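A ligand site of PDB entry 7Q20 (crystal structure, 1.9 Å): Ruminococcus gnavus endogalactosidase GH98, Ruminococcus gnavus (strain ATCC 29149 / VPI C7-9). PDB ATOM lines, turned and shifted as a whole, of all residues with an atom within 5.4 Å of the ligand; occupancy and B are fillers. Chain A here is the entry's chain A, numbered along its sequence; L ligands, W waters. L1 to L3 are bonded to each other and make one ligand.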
ATOM      1  N   TYR A 242       5.137 -37.055   0.516  1.00  0.00           N
ATOM      2  CA  TYR A 242       5.725 -36.456   1.732  1.00  0.00           C
ATOM      3  C   TYR A 242       5.546 -37.406   2.925  1.00  0.00           C
ATOM      4  O   TYR A 242       4.409 -37.794   3.207  1.00  0.00           O
ATOM      5  CB  TYR A 242       5.074 -35.124   2.076  1.00  0.00           C
ATOM      6  CG  TYR A 242       5.512 -33.961   1.229  1.00  0.00           C
ATOM      7  CD1 TYR A 242       6.765 -33.387   1.401  1.00  0.00           C
ATOM      8  CD2 TYR A 242       4.688 -33.447   0.253  1.00  0.00           C
ATOM      9  CE1 TYR A 242       7.170 -32.314   0.627  1.00  0.00           C
ATOM     10  CE2 TYR A 242       5.085 -32.377  -0.532  1.00  0.00           C
ATOM     11  CZ  TYR A 242       6.337 -31.811  -0.348  1.00  0.00           C
ATOM     12  OH  TYR A 242       6.754 -30.747  -1.093  1.00  0.00           O
ATOM     13  N   GLN A 258       1.736 -37.720   4.202  1.00  0.00           N
ATOM     14  CA  GLN A 258       0.738 -36.689   4.470  1.00  0.00           C
ATOM     15  C   GLN A 258      -0.631 -37.146   3.978  1.00  0.00           C
ATOM     16  O   GLN A 258      -0.737 -37.837   2.959  1.00  0.00           O
ATOM     17  CB  GLN A 258       1.143 -35.382   3.786  1.00  0.00           C
ATOM     18  CG  GLN A 258       2.334 -34.680   4.428  1.00  0.00           C
ATOM     19  CD  GLN A 258       2.581 -33.271   3.899  1.00  0.00           C
ATOM     20  OE1 GLN A 258       3.216 -32.465   4.587  1.00  0.00           O
ATOM     21  NE2 GLN A 258       2.077 -32.944   2.693  1.00  0.00           N
ATOM     22  N   HIS A 283       9.763 -37.939  -0.425  1.00  0.00           N
ATOM     23  CA  HIS A 283      10.242 -36.681   0.169  1.00  0.00           C
ATOM     24  C   HIS A 283      10.201 -36.833   1.695  1.00  0.00           C
ATOM     25  O   HIS A 283       9.151 -37.132   2.272  1.00  0.00           O
ATOM     26  CB  HIS A 283       9.359 -35.517  -0.315  1.00  0.00           C
ATOM     27  CG  HIS A 283       9.916 -34.147  -0.063  1.00  0.00           C
ATOM     28  ND1 HIS A 283      10.276 -33.702   1.186  1.00  0.00           N
ATOM     29  CD2 HIS A 283      10.107 -33.093  -0.902  1.00  0.00           C
ATOM     30  CE1 HIS A 283      10.691 -32.440   1.116  1.00  0.00           C
ATOM     31  NE2 HIS A 283      10.606 -32.046  -0.145  1.00  0.00           N
ATOM     32  N   ASN A 285      10.484 -34.633   3.985  1.00  0.00           N
ATOM     33  CA  ASN A 285       9.691 -33.605   4.648  1.00  0.00           C
ATOM     34  C   ASN A 285      10.482 -33.207   5.897  1.00  0.00           C
ATOM     35  O   ASN A 285      11.689 -33.006   5.801  1.00  0.00           O
ATOM     36  CB  ASN A 285       8.284 -34.140   4.928  1.00  0.00           C
ATOM     37  CG  ASN A 285       7.264 -33.037   5.095  1.00  0.00           C
ATOM     38  OD1 ASN A 285       7.539 -31.849   4.834  1.00  0.00           O
ATOM     39  ND2 ASN A 285       6.078 -33.421   5.533  1.00  0.00           N
ATOM     40  N   ASN A 286       9.830 -33.158   7.068  1.00  0.00           N
ATOM     41  CA  ASN A 286      10.490 -32.765   8.314  1.00  0.00           C
ATOM     42  C   ASN A 286      10.798 -33.959   9.253  1.00  0.00           C
ATOM     43  O   ASN A 286      10.954 -33.790  10.452  1.00  0.00           O
ATOM     44  CB  ASN A 286       9.672 -31.684   8.999  1.00  0.00           C
ATOM     45  CG  ASN A 286       9.589 -30.422   8.157  1.00  0.00           C
ATOM     46  OD1 ASN A 286       8.506 -29.833   7.962  1.00  0.00           O
ATOM     47  ND2 ASN A 286      10.736 -29.978   7.642  1.00  0.00           N
ATOM     48  N   LEU A 321      14.161 -37.493  -3.068  1.00  0.00           N
ATOM     49  CA  LEU A 321      14.656 -36.185  -2.702  1.00  0.00           C
ATOM     50  C   LEU A 321      16.106 -36.320  -2.265  1.00  0.00           C
ATOM     51  O   LEU A 321      16.411 -37.024  -1.325  1.00  0.00           O
ATOM     52  CB  LEU A 321      13.864 -35.609  -1.543  1.00  0.00           C
ATOM     53  CG  LEU A 321      14.314 -34.201  -1.128  1.00  0.00           C
ATOM     54  CD1 LEU A 321      13.944 -33.188  -2.216  1.00  0.00           C
ATOM     55  CD2 LEU A 321      13.734 -33.827   0.209  1.00  0.00           C
ATOM     56  N   THR A 324      17.477 -30.556  -0.423  1.00  0.00           N
ATOM     57  CA  THR A 324      16.640 -29.371  -0.256  1.00  0.00           C
ATOM     58  C   THR A 324      17.223 -28.561   0.884  1.00  0.00           C
ATOM     59  O   THR A 324      17.931 -29.101   1.735  1.00  0.00           O
ATOM     60  CB  THR A 324      15.161 -29.738  -0.004  1.00  0.00           C
ATOM     61  OG1 THR A 324      14.336 -28.588  -0.136  1.00  0.00           O
ATOM     62  CG2 THR A 324      14.961 -30.353   1.391  1.00  0.00           C
ATOM     63  N   ALA A 325      16.947 -27.252   0.881  1.00  0.00           N
ATOM     64  CA  ALA A 325      17.348 -26.339   1.945  1.00  0.00           C
ATOM     65  C   ALA A 325      18.862 -26.338   2.249  1.00  0.00           C
ATOM     66  O   ALA A 325      19.277 -26.035   3.381  1.00  0.00           O
ATOM     67  CB  ALA A 325      16.531 -26.623   3.193  1.00  0.00           C
ATOM     68  N   THR A 363      15.432 -29.152  -4.809  1.00  0.00           N
ATOM     69  CA  THR A 363      14.672 -27.912  -4.824  1.00  0.00           C
ATOM     70  C   THR A 363      14.941 -27.043  -3.612  1.00  0.00           C
ATOM     71  O   THR A 363      15.278 -27.541  -2.536  1.00  0.00           O
ATOM     72  CB  THR A 363      13.144 -28.186  -4.933  1.00  0.00           C
ATOM     73  OG1 THR A 363      12.429 -26.959  -5.162  1.00  0.00           O
ATOM     74  CG2 THR A 363      12.613 -28.823  -3.670  1.00  0.00           C
ATOM     75  N   GLU A 364      14.774 -25.728  -3.807  1.00  0.00           N
ATOM     76  CA  GLU A 364      14.720 -24.746  -2.733  1.00  0.00           C
ATOM     77  C   GLU A 364      15.966 -24.807  -1.861  1.00  0.00           C
ATOM     78  O   GLU A 364      15.872 -25.023  -0.644  1.00  0.00           O
ATOM     79  CB  GLU A 364      13.468 -24.953  -1.878  1.00  0.00           C
ATOM     80  CG  GLU A 364      12.151 -24.590  -2.574  1.00  0.00           C
ATOM     81  CD  GLU A 364      11.890 -23.107  -2.641  1.00  0.00           C
ATOM     82  OE1 GLU A 364      12.652 -22.314  -2.030  1.00  0.00           O
ATOM     83  OE2 GLU A 364      10.919 -22.721  -3.321  1.00  0.00           O
ATOM     84  N   TRP A 367      18.286 -20.105  -0.979  1.00  0.00           N
ATOM     85  CA  TRP A 367      17.991 -19.236   0.144  1.00  0.00           C
ATOM     86  C   TRP A 367      18.899 -19.567   1.348  1.00  0.00           C
ATOM     87  O   TRP A 367      19.140 -18.720   2.198  1.00  0.00           O
ATOM     88  CB  TRP A 367      16.506 -19.295   0.523  1.00  0.00           C
ATOM     89  CG  TRP A 367      16.068 -20.648   1.030  1.00  0.00           C
ATOM     90  CD1 TRP A 367      15.624 -21.706   0.291  1.00  0.00           C
ATOM     91  CD2 TRP A 367      16.064 -21.090   2.393  1.00  0.00           C
ATOM     92  NE1 TRP A 367      15.348 -22.788   1.126  1.00  0.00           N
ATOM     93  CE2 TRP A 367      15.591 -22.416   2.414  1.00  0.00           C
ATOM     94  CE3 TRP A 367      16.403 -20.474   3.613  1.00  0.00           C
ATOM     95  CZ2 TRP A 367      15.460 -23.144   3.587  1.00  0.00           C
ATOM     96  CZ3 TRP A 367      16.251 -21.193   4.780  1.00  0.00           C
ATOM     97  CH2 TRP A 367      15.785 -22.519   4.761  1.00  0.00           C
ATOM     98  N   LYS A 427       9.026 -23.299 -10.358  1.00  0.00           N
ATOM     99  CA  LYS A 427       8.377 -23.476  -9.070  1.00  0.00           C
ATOM    100  C   LYS A 427       7.817 -22.126  -8.636  1.00  0.00           C
ATOM    101  O   LYS A 427       8.568 -21.275  -8.183  1.00  0.00           O
ATOM    102  CB  LYS A 427       9.398 -23.984  -8.057  1.00  0.00           C
ATOM    103  CG  LYS A 427       8.798 -24.404  -6.714  1.00  0.00           C
ATOM    104  CD  LYS A 427       9.808 -25.190  -5.905  1.00  0.00           C
ATOM    105  CE  LYS A 427       9.220 -25.658  -4.567  1.00  0.00           C
ATOM    106  NZ  LYS A 427       8.912 -24.539  -3.632  1.00  0.00           N
ATOM    107  N   THR A 429       5.881 -21.070  -6.204  1.00  0.00           N
ATOM    108  CA  THR A 429       5.572 -20.851  -4.779  1.00  0.00           C
ATOM    109  C   THR A 429       5.553 -19.373  -4.388  1.00  0.00           C
ATOM    110  O   THR A 429       4.555 -18.890  -3.829  1.00  0.00           O
ATOM    111  CB  THR A 429       6.580 -21.613  -3.913  1.00  0.00           C
ATOM    112  OG1 THR A 429       6.581 -22.972  -4.332  1.00  0.00           O
ATOM    113  CG2 THR A 429       6.247 -21.542  -2.443  1.00  0.00           C
ATOM    114  N   ASP A 460       2.354 -24.728  -7.832  1.00  0.00           N
ATOM    115  CA  ASP A 460       2.191 -24.870  -6.391  1.00  0.00           C
ATOM    116  C   ASP A 460       0.985 -24.006  -6.004  1.00  0.00           C
ATOM    117  O   ASP A 460       0.965 -22.809  -6.272  1.00  0.00           O
ATOM    118  CB  ASP A 460       3.474 -24.382  -5.696  1.00  0.00           C
ATOM    119  CG  ASP A 460       3.529 -24.728  -4.223  1.00  0.00           C
ATOM    120  OD1 ASP A 460       2.498 -25.139  -3.648  1.00  0.00           O
ATOM    121  OD2 ASP A 460       4.632 -24.599  -3.645  1.00  0.00           O
ATOM    122  N   TRP A 462       0.527 -22.987  -3.144  1.00  0.00           N
ATOM    123  CA  TRP A 462       1.085 -21.941  -2.296  1.00  0.00           C
ATOM    124  C   TRP A 462       1.109 -20.588  -3.033  1.00  0.00           C
ATOM    125  O   TRP A 462       1.059 -19.536  -2.395  1.00  0.00           O
ATOM    126  CB  TRP A 462       2.499 -22.285  -1.752  1.00  0.00           C
ATOM    127  CG  TRP A 462       2.506 -23.242  -0.556  1.00  0.00           C
ATOM    128  CD1 TRP A 462       3.081 -24.474  -0.492  1.00  0.00           C
ATOM    129  CD2 TRP A 462       1.925 -23.002   0.745  1.00  0.00           C
ATOM    130  NE1 TRP A 462       2.887 -25.025   0.768  1.00  0.00           N
ATOM    131  CE2 TRP A 462       2.180 -24.137   1.539  1.00  0.00           C
ATOM    132  CE3 TRP A 462       1.221 -21.926   1.307  1.00  0.00           C
ATOM    133  CZ2 TRP A 462       1.732 -24.255   2.856  1.00  0.00           C
ATOM    134  CZ3 TRP A 462       0.786 -22.020   2.583  1.00  0.00           C
ATOM    135  CH2 TRP A 462       1.047 -23.189   3.372  1.00  0.00           C
ATOM    136  N   ASP A 465      -1.822 -18.484  -1.975  1.00  0.00           N
ATOM    137  CA  ASP A 465      -1.616 -17.951  -0.623  1.00  0.00           C
ATOM    138  C   ASP A 465      -1.000 -16.570  -0.608  1.00  0.00           C
ATOM    139  O   ASP A 465      -1.312 -15.767   0.252  1.00  0.00           O
ATOM    140  CB  ASP A 465      -0.728 -18.902   0.218  1.00  0.00           C
ATOM    141  CG  ASP A 465      -0.290 -18.302   1.575  1.00  0.00           C
ATOM    142  OD1 ASP A 465      -1.150 -17.791   2.340  1.00  0.00           O
ATOM    143  OD2 ASP A 465       0.911 -18.379   1.916  1.00  0.00           O
ATOM    144  N   LYS A 466      -0.107 -16.311  -1.568  1.00  0.00           N
ATOM    145  CA  LYS A 466       0.653 -15.063  -1.603  1.00  0.00           C
ATOM    146  C   LYS A 466      -0.160 -13.878  -2.124  1.00  0.00           C
ATOM    147  O   LYS A 466       0.286 -12.748  -1.988  1.00  0.00           O
ATOM    148  CB  LYS A 466       1.926 -15.229  -2.456  1.00  0.00           C
ATOM    149  CG  LYS A 466       2.791 -16.433  -2.109  1.00  0.00           C
ATOM    150  CD  LYS A 466       3.438 -16.307  -0.732  1.00  0.00           C
ATOM    151  CE  LYS A 466       4.340 -17.509  -0.437  1.00  0.00           C
ATOM    152  NZ  LYS A 466       3.568 -18.632   0.131  1.00  0.00           N
ATOM    153  N   TRP A 481      -3.074 -21.725   5.531  1.00  0.00           N
ATOM    154  CA  TRP A 481      -3.623 -23.050   5.190  1.00  0.00           C
ATOM    155  C   TRP A 481      -5.002 -22.982   4.517  1.00  0.00           C
ATOM    156  O   TRP A 481      -5.333 -23.850   3.710  1.00  0.00           O
ATOM    157  CB  TRP A 481      -3.596 -24.022   6.421  1.00  0.00           C
ATOM    158  CG  TRP A 481      -2.182 -24.289   6.829  1.00  0.00           C
ATOM    159  CD1 TRP A 481      -1.478 -23.644   7.811  1.00  0.00           C
ATOM    160  CD2 TRP A 481      -1.254 -25.197   6.217  1.00  0.00           C
ATOM    161  NE1 TRP A 481      -0.203 -24.108   7.864  1.00  0.00           N
ATOM    162  CE2 TRP A 481      -0.033 -25.064   6.896  1.00  0.00           C
ATOM    163  CE3 TRP A 481      -1.344 -26.114   5.183  1.00  0.00           C
ATOM    164  CZ2 TRP A 481       1.092 -25.804   6.570  1.00  0.00           C
ATOM    165  CZ3 TRP A 481      -0.207 -26.864   4.850  1.00  0.00           C
ATOM    166  CH2 TRP A 481       0.986 -26.695   5.541  1.00  0.00           C
ATOM    167  N   GLU A 510       1.718 -29.225  -6.444  1.00  0.00           N
ATOM    168  CA  GLU A 510       1.578 -29.195  -4.975  1.00  0.00           C
ATOM    169  C   GLU A 510       0.459 -28.188  -4.722  1.00  0.00           C
ATOM    170  O   GLU A 510       0.210 -27.359  -5.591  1.00  0.00           O
ATOM    171  CB  GLU A 510       2.863 -28.730  -4.338  1.00  0.00           C
ATOM    172  CG  GLU A 510       4.048 -29.558  -4.772  1.00  0.00           C
ATOM    173  CD  GLU A 510       5.149 -29.557  -3.745  1.00  0.00           C
ATOM    174  OE1 GLU A 510       4.931 -30.175  -2.725  1.00  0.00           O
ATOM    175  OE2 GLU A 510       6.193 -28.898  -3.942  1.00  0.00           O
ATOM    176  N   PHE A 511      -0.207 -28.203  -3.560  1.00  0.00           N
ATOM    177  CA  PHE A 511      -0.023 -29.112  -2.421  1.00  0.00           C
ATOM    178  C   PHE A 511      -0.582 -30.486  -2.777  1.00  0.00           C
ATOM    179  O   PHE A 511      -1.730 -30.594  -3.171  1.00  0.00           O
ATOM    180  CB  PHE A 511      -0.836 -28.499  -1.257  1.00  0.00           C
ATOM    181  CG  PHE A 511      -0.664 -29.167   0.094  1.00  0.00           C
ATOM    182  CD1 PHE A 511       0.480 -28.990   0.825  1.00  0.00           C
ATOM    183  CD2 PHE A 511      -1.743 -29.839   0.691  1.00  0.00           C
ATOM    184  CE1 PHE A 511       0.608 -29.556   2.109  1.00  0.00           C
ATOM    185  CE2 PHE A 511      -1.629 -30.402   1.958  1.00  0.00           C
ATOM    186  CZ  PHE A 511      -0.451 -30.267   2.667  1.00  0.00           C
ATOM    187  N   PRO A 512       0.203 -31.581  -2.641  1.00  0.00           N
ATOM    188  CA  PRO A 512      -0.196 -32.879  -3.182  1.00  0.00           C
ATOM    189  C   PRO A 512      -1.546 -33.396  -2.655  1.00  0.00           C
ATOM    190  O   PRO A 512      -2.271 -34.010  -3.401  1.00  0.00           O
ATOM    191  CB  PRO A 512       0.930 -33.817  -2.733  1.00  0.00           C
ATOM    192  CG  PRO A 512       2.109 -32.917  -2.514  1.00  0.00           C
ATOM    193  CD  PRO A 512       1.507 -31.637  -1.961  1.00  0.00           C
ATOM    194  N   ILE A 738       0.279 -30.237  12.546  1.00  0.00           N
ATOM    195  CA  ILE A 738      -0.373 -28.973  12.863  1.00  0.00           C
ATOM    196  C   ILE A 738      -1.818 -28.914  12.336  1.00  0.00           C
ATOM    197  O   ILE A 738      -2.180 -29.545  11.331  1.00  0.00           O
ATOM    198  CB  ILE A 738       0.452 -27.741  12.371  1.00  0.00           C
ATOM    199  CG1 ILE A 738       0.576 -27.741  10.844  1.00  0.00           C
ATOM    200  CG2 ILE A 738       1.849 -27.761  13.002  1.00  0.00           C
ATOM    201  CD1 ILE A 738       1.212 -26.475  10.273  1.00  0.00           C
ATOM    202  N   LYS A 741      -2.900 -28.138   8.593  1.00  0.00           N
ATOM    203  CA  LYS A 741      -2.738 -29.302   7.720  1.00  0.00           C
ATOM    204  C   LYS A 741      -3.859 -30.320   7.914  1.00  0.00           C
ATOM    205  O   LYS A 741      -4.432 -30.826   6.937  1.00  0.00           O
ATOM    206  CB  LYS A 741      -1.402 -29.993   7.966  1.00  0.00           C
ATOM    207  CG  LYS A 741      -0.214 -29.386   7.265  1.00  0.00           C
ATOM    208  CD  LYS A 741       0.969 -30.315   7.424  1.00  0.00           C
ATOM    209  CE  LYS A 741       2.099 -29.933   6.513  1.00  0.00           C
ATOM    210  NZ  LYS A 741       3.371 -30.595   6.920  1.00  0.00           N
HETATM  211  C1  LIG L   1       8.868 -27.219   1.731  1.00  0.00           C
HETATM  212  C2  LIG L   1       8.948 -28.426   0.820  1.00  0.00           C
HETATM  213  C3  LIG L   1       9.883 -28.168  -0.355  1.00  0.00           C
HETATM  214  C4  LIG L   1      11.249 -27.718   0.149  1.00  0.00           C
HETATM  215  C5  LIG L   1      11.074 -26.519   1.085  1.00  0.00           C
HETATM  216  C6  LIG L   1      12.386 -26.061   1.705  1.00  0.00           C
HETATM  217  O1  LIG L   1       7.619 -28.735   0.368  1.00  0.00           O
HETATM  218  O2  LIG L   1      10.005 -29.350  -1.152  1.00  0.00           O
HETATM  219  O3  LIG L   1      11.911 -28.806   0.831  1.00  0.00           O
HETATM  220  O4  LIG L   1      10.170 -26.830   2.145  1.00  0.00           O
HETATM  221  C1  LG2 L   2       7.804 -23.790   0.878  1.00  0.00           C
HETATM  222  C2  LG2 L   2       7.646 -25.002   1.815  1.00  0.00           C
HETATM  223  C3  LG2 L   2       6.201 -25.179   2.284  1.00  0.00           C
HETATM  224  C4  LG2 L   2       5.636 -23.858   2.800  1.00  0.00           C
HETATM  225  C5  LG2 L   2       5.837 -22.778   1.752  1.00  0.00           C
HETATM  226  C6  LG2 L   2       5.231 -21.443   2.205  1.00  0.00           C
HETATM  227  O1  LG2 L   2       9.194 -23.572   0.639  1.00  0.00           O
HETATM  228  O2  LG2 L   2       8.050 -26.186   1.129  1.00  0.00           O
HETATM  229  O3  LG2 L   2       6.115 -26.194   3.288  1.00  0.00           O
HETATM  230  O4  LG2 L   2       6.273 -23.503   4.036  1.00  0.00           O
HETATM  231  O5  LG2 L   2       7.235 -22.625   1.481  1.00  0.00           O
HETATM  232  O6  LG2 L   2       5.065 -20.557   1.095  1.00  0.00           O
HETATM  233  O1  LG3 L   3       4.177 -27.340   2.587  1.00  0.00           O
HETATM  234  C1  LG3 L   3       4.881 -26.766   3.676  1.00  0.00           C
HETATM  235  C2  LG3 L   3       5.047 -27.793   4.797  1.00  0.00           C
HETATM  236  N1  LG3 L   3       5.783 -27.238   5.902  1.00  0.00           N
HETATM  237  C3  LG3 L   3       5.708 -29.067   4.272  1.00  0.00           C
HETATM  238  O2  LG3 L   3       5.651 -30.051   5.291  1.00  0.00           O
HETATM  239  C4  LG3 L   3       5.038 -29.576   3.001  1.00  0.00           C
HETATM  240  O3  LG3 L   3       3.751 -30.094   3.325  1.00  0.00           O
HETATM  241  C5  LG3 L   3       4.897 -28.442   1.986  1.00  0.00           C
HETATM  242  C6  LG3 L   3       4.117 -28.821   0.741  1.00  0.00           C
HETATM  243  O4  LG3 L   3       3.893 -27.678  -0.094  1.00  0.00           O
HETATM  244  C7  LG3 L   3       5.367 -27.274   7.176  1.00  0.00           C
HETATM  245  O5  LG3 L   3       4.314 -27.812   7.490  1.00  0.00           O
HETATM  246  C8  LG3 L   3       6.278 -26.643   8.184  1.00  0.00           C
HETATM  247  O   HOH W   1       9.043 -27.374   5.686  1.00  0.00           O
HETATM  248  O   HOH W   2      11.504 -29.786   3.190  1.00  0.00           O
HETATM  249  O   HOH W   3       6.307 -26.635  -1.894  1.00  0.00           O
HETATM  250  O   HOH W   4       8.672 -29.359  -3.631  1.00  0.00           O
HETATM  251  O   HOH W   5       6.328 -31.034   8.470  1.00  0.00           O
HETATM  252  O   HOH W   6       8.093 -25.011   5.973  1.00  0.00           O
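The side-chain hydroxyl (OG1) of Thr 324 is in hydrogen-bond range of an oxygen (O3) of LIG L1, 2.6 Å away.
An oxygen (O6) of LG2 L2 lies within hydrogen-bond range of the side-chain amino group (NZ) of Lys 466.
An oxygen (O1) of LIG L1 sits at hydrogen-bond distance from the side-chain hydroxyl of Tyr 242, 2.6 Å away.
The side-chain amide oxygen (OD1) of Asn 285 is in hydrogen-bond range of an oxygen (O2) of LG3 L3 (2.6 Å).
OE1 of Gln 258 sits at hydrogen-bond distance from O3 of LG3 L3 (2.7 Å).
NZ of Lys 741 is in hydrogen-bond range of O2 of LG3 L3 (2.9 Å).
NE2 of His 283 lies within hydrogen-bond range of O2 of LIG L1, at 2.9 Å.
The indole nitrogen of Trp 462 lies within hydrogen-bond range of an oxygen (O4) of LG3 L3.
Asn 286 touches the ligand.
CG2 of Thr 363 touches O2 of LIG L1, 3.7 Å away.
Glu 364 touches the ligand.
CG2 of Thr 429 touches O6 of LG2 L2, at 3.9 Å.
CZ2 of Trp 481 touches O5 of LG3 L3, at 3.9 Å.
Glu 510 touches the ligand.
CE1 of Phe 511 touches O3 of LG3 L3, 3.4 Å away.
Hydrophobic or aromatic side chains within 4 Å of the ligand: Tyr 242, His 283, Trp 462, Trp 481 and Phe 511.
Within 4 Å of the ligand: Tyr 242, Gln 258, His 283, Asn 285, Asn 286, Thr 324, Thr 363, Glu 364, Thr 429, Trp 462, Lys 466, Trp 481, Glu 510, Phe 511 and Lys 741.
The nearest printed residue that does not touch the ligand is Ile 738 (4.4 Å).
OG1 of Thr 324 is in hydrogen-bond range of O of Thr 363, at 2.8 Å.
O of Tyr 242 sits at hydrogen-bond distance from N of Gln 258 (2.9 Å).
OH of Tyr 242 lies within hydrogen-bond range of OE1 of Glu 510.
The backbone NH (N) of Trp 462 sits at hydrogen-bond distance from the side-chain carboxylate (OD1) of Asp 460 (3.0 Å).
OG1 of Thr 429 sits at hydrogen-bond distance from NZ of Lys 427 (2.9 Å).
OE2 of Glu 364 lies within salt-bridge range of NZ of Lys 427 (2.7 Å).
N of Ala 325 is in hydrogen-bond range of O of Glu 364, at 2.9 Å.
The indole nitrogen (NE1) of Trp 367 is in hydrogen-bond range of the backbone carbonyl oxygen (O) of Glu 364 (2.9 Å).
Water W4 lies within hydrogen-bond range of OE2 of Glu 510, O2 of LIG L1 and OH of Tyr 242.
Water W3 lies within hydrogen-bond range of the side-chain carboxylate (OE2) of Glu 510, the side-chain carboxylate (OD2) of Asp 460 and an oxygen (O4) of LG3 L3.
Water W1 bridges N1 of LG3 L3 and OD1 of Asn 286.
Water W5 lies within hydrogen-bond range of OD1 of Asn 286 (2.5 Å), NZ of Lys 741 (3.4 Å) and O2 of LG3 L3 (3.4 Å).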
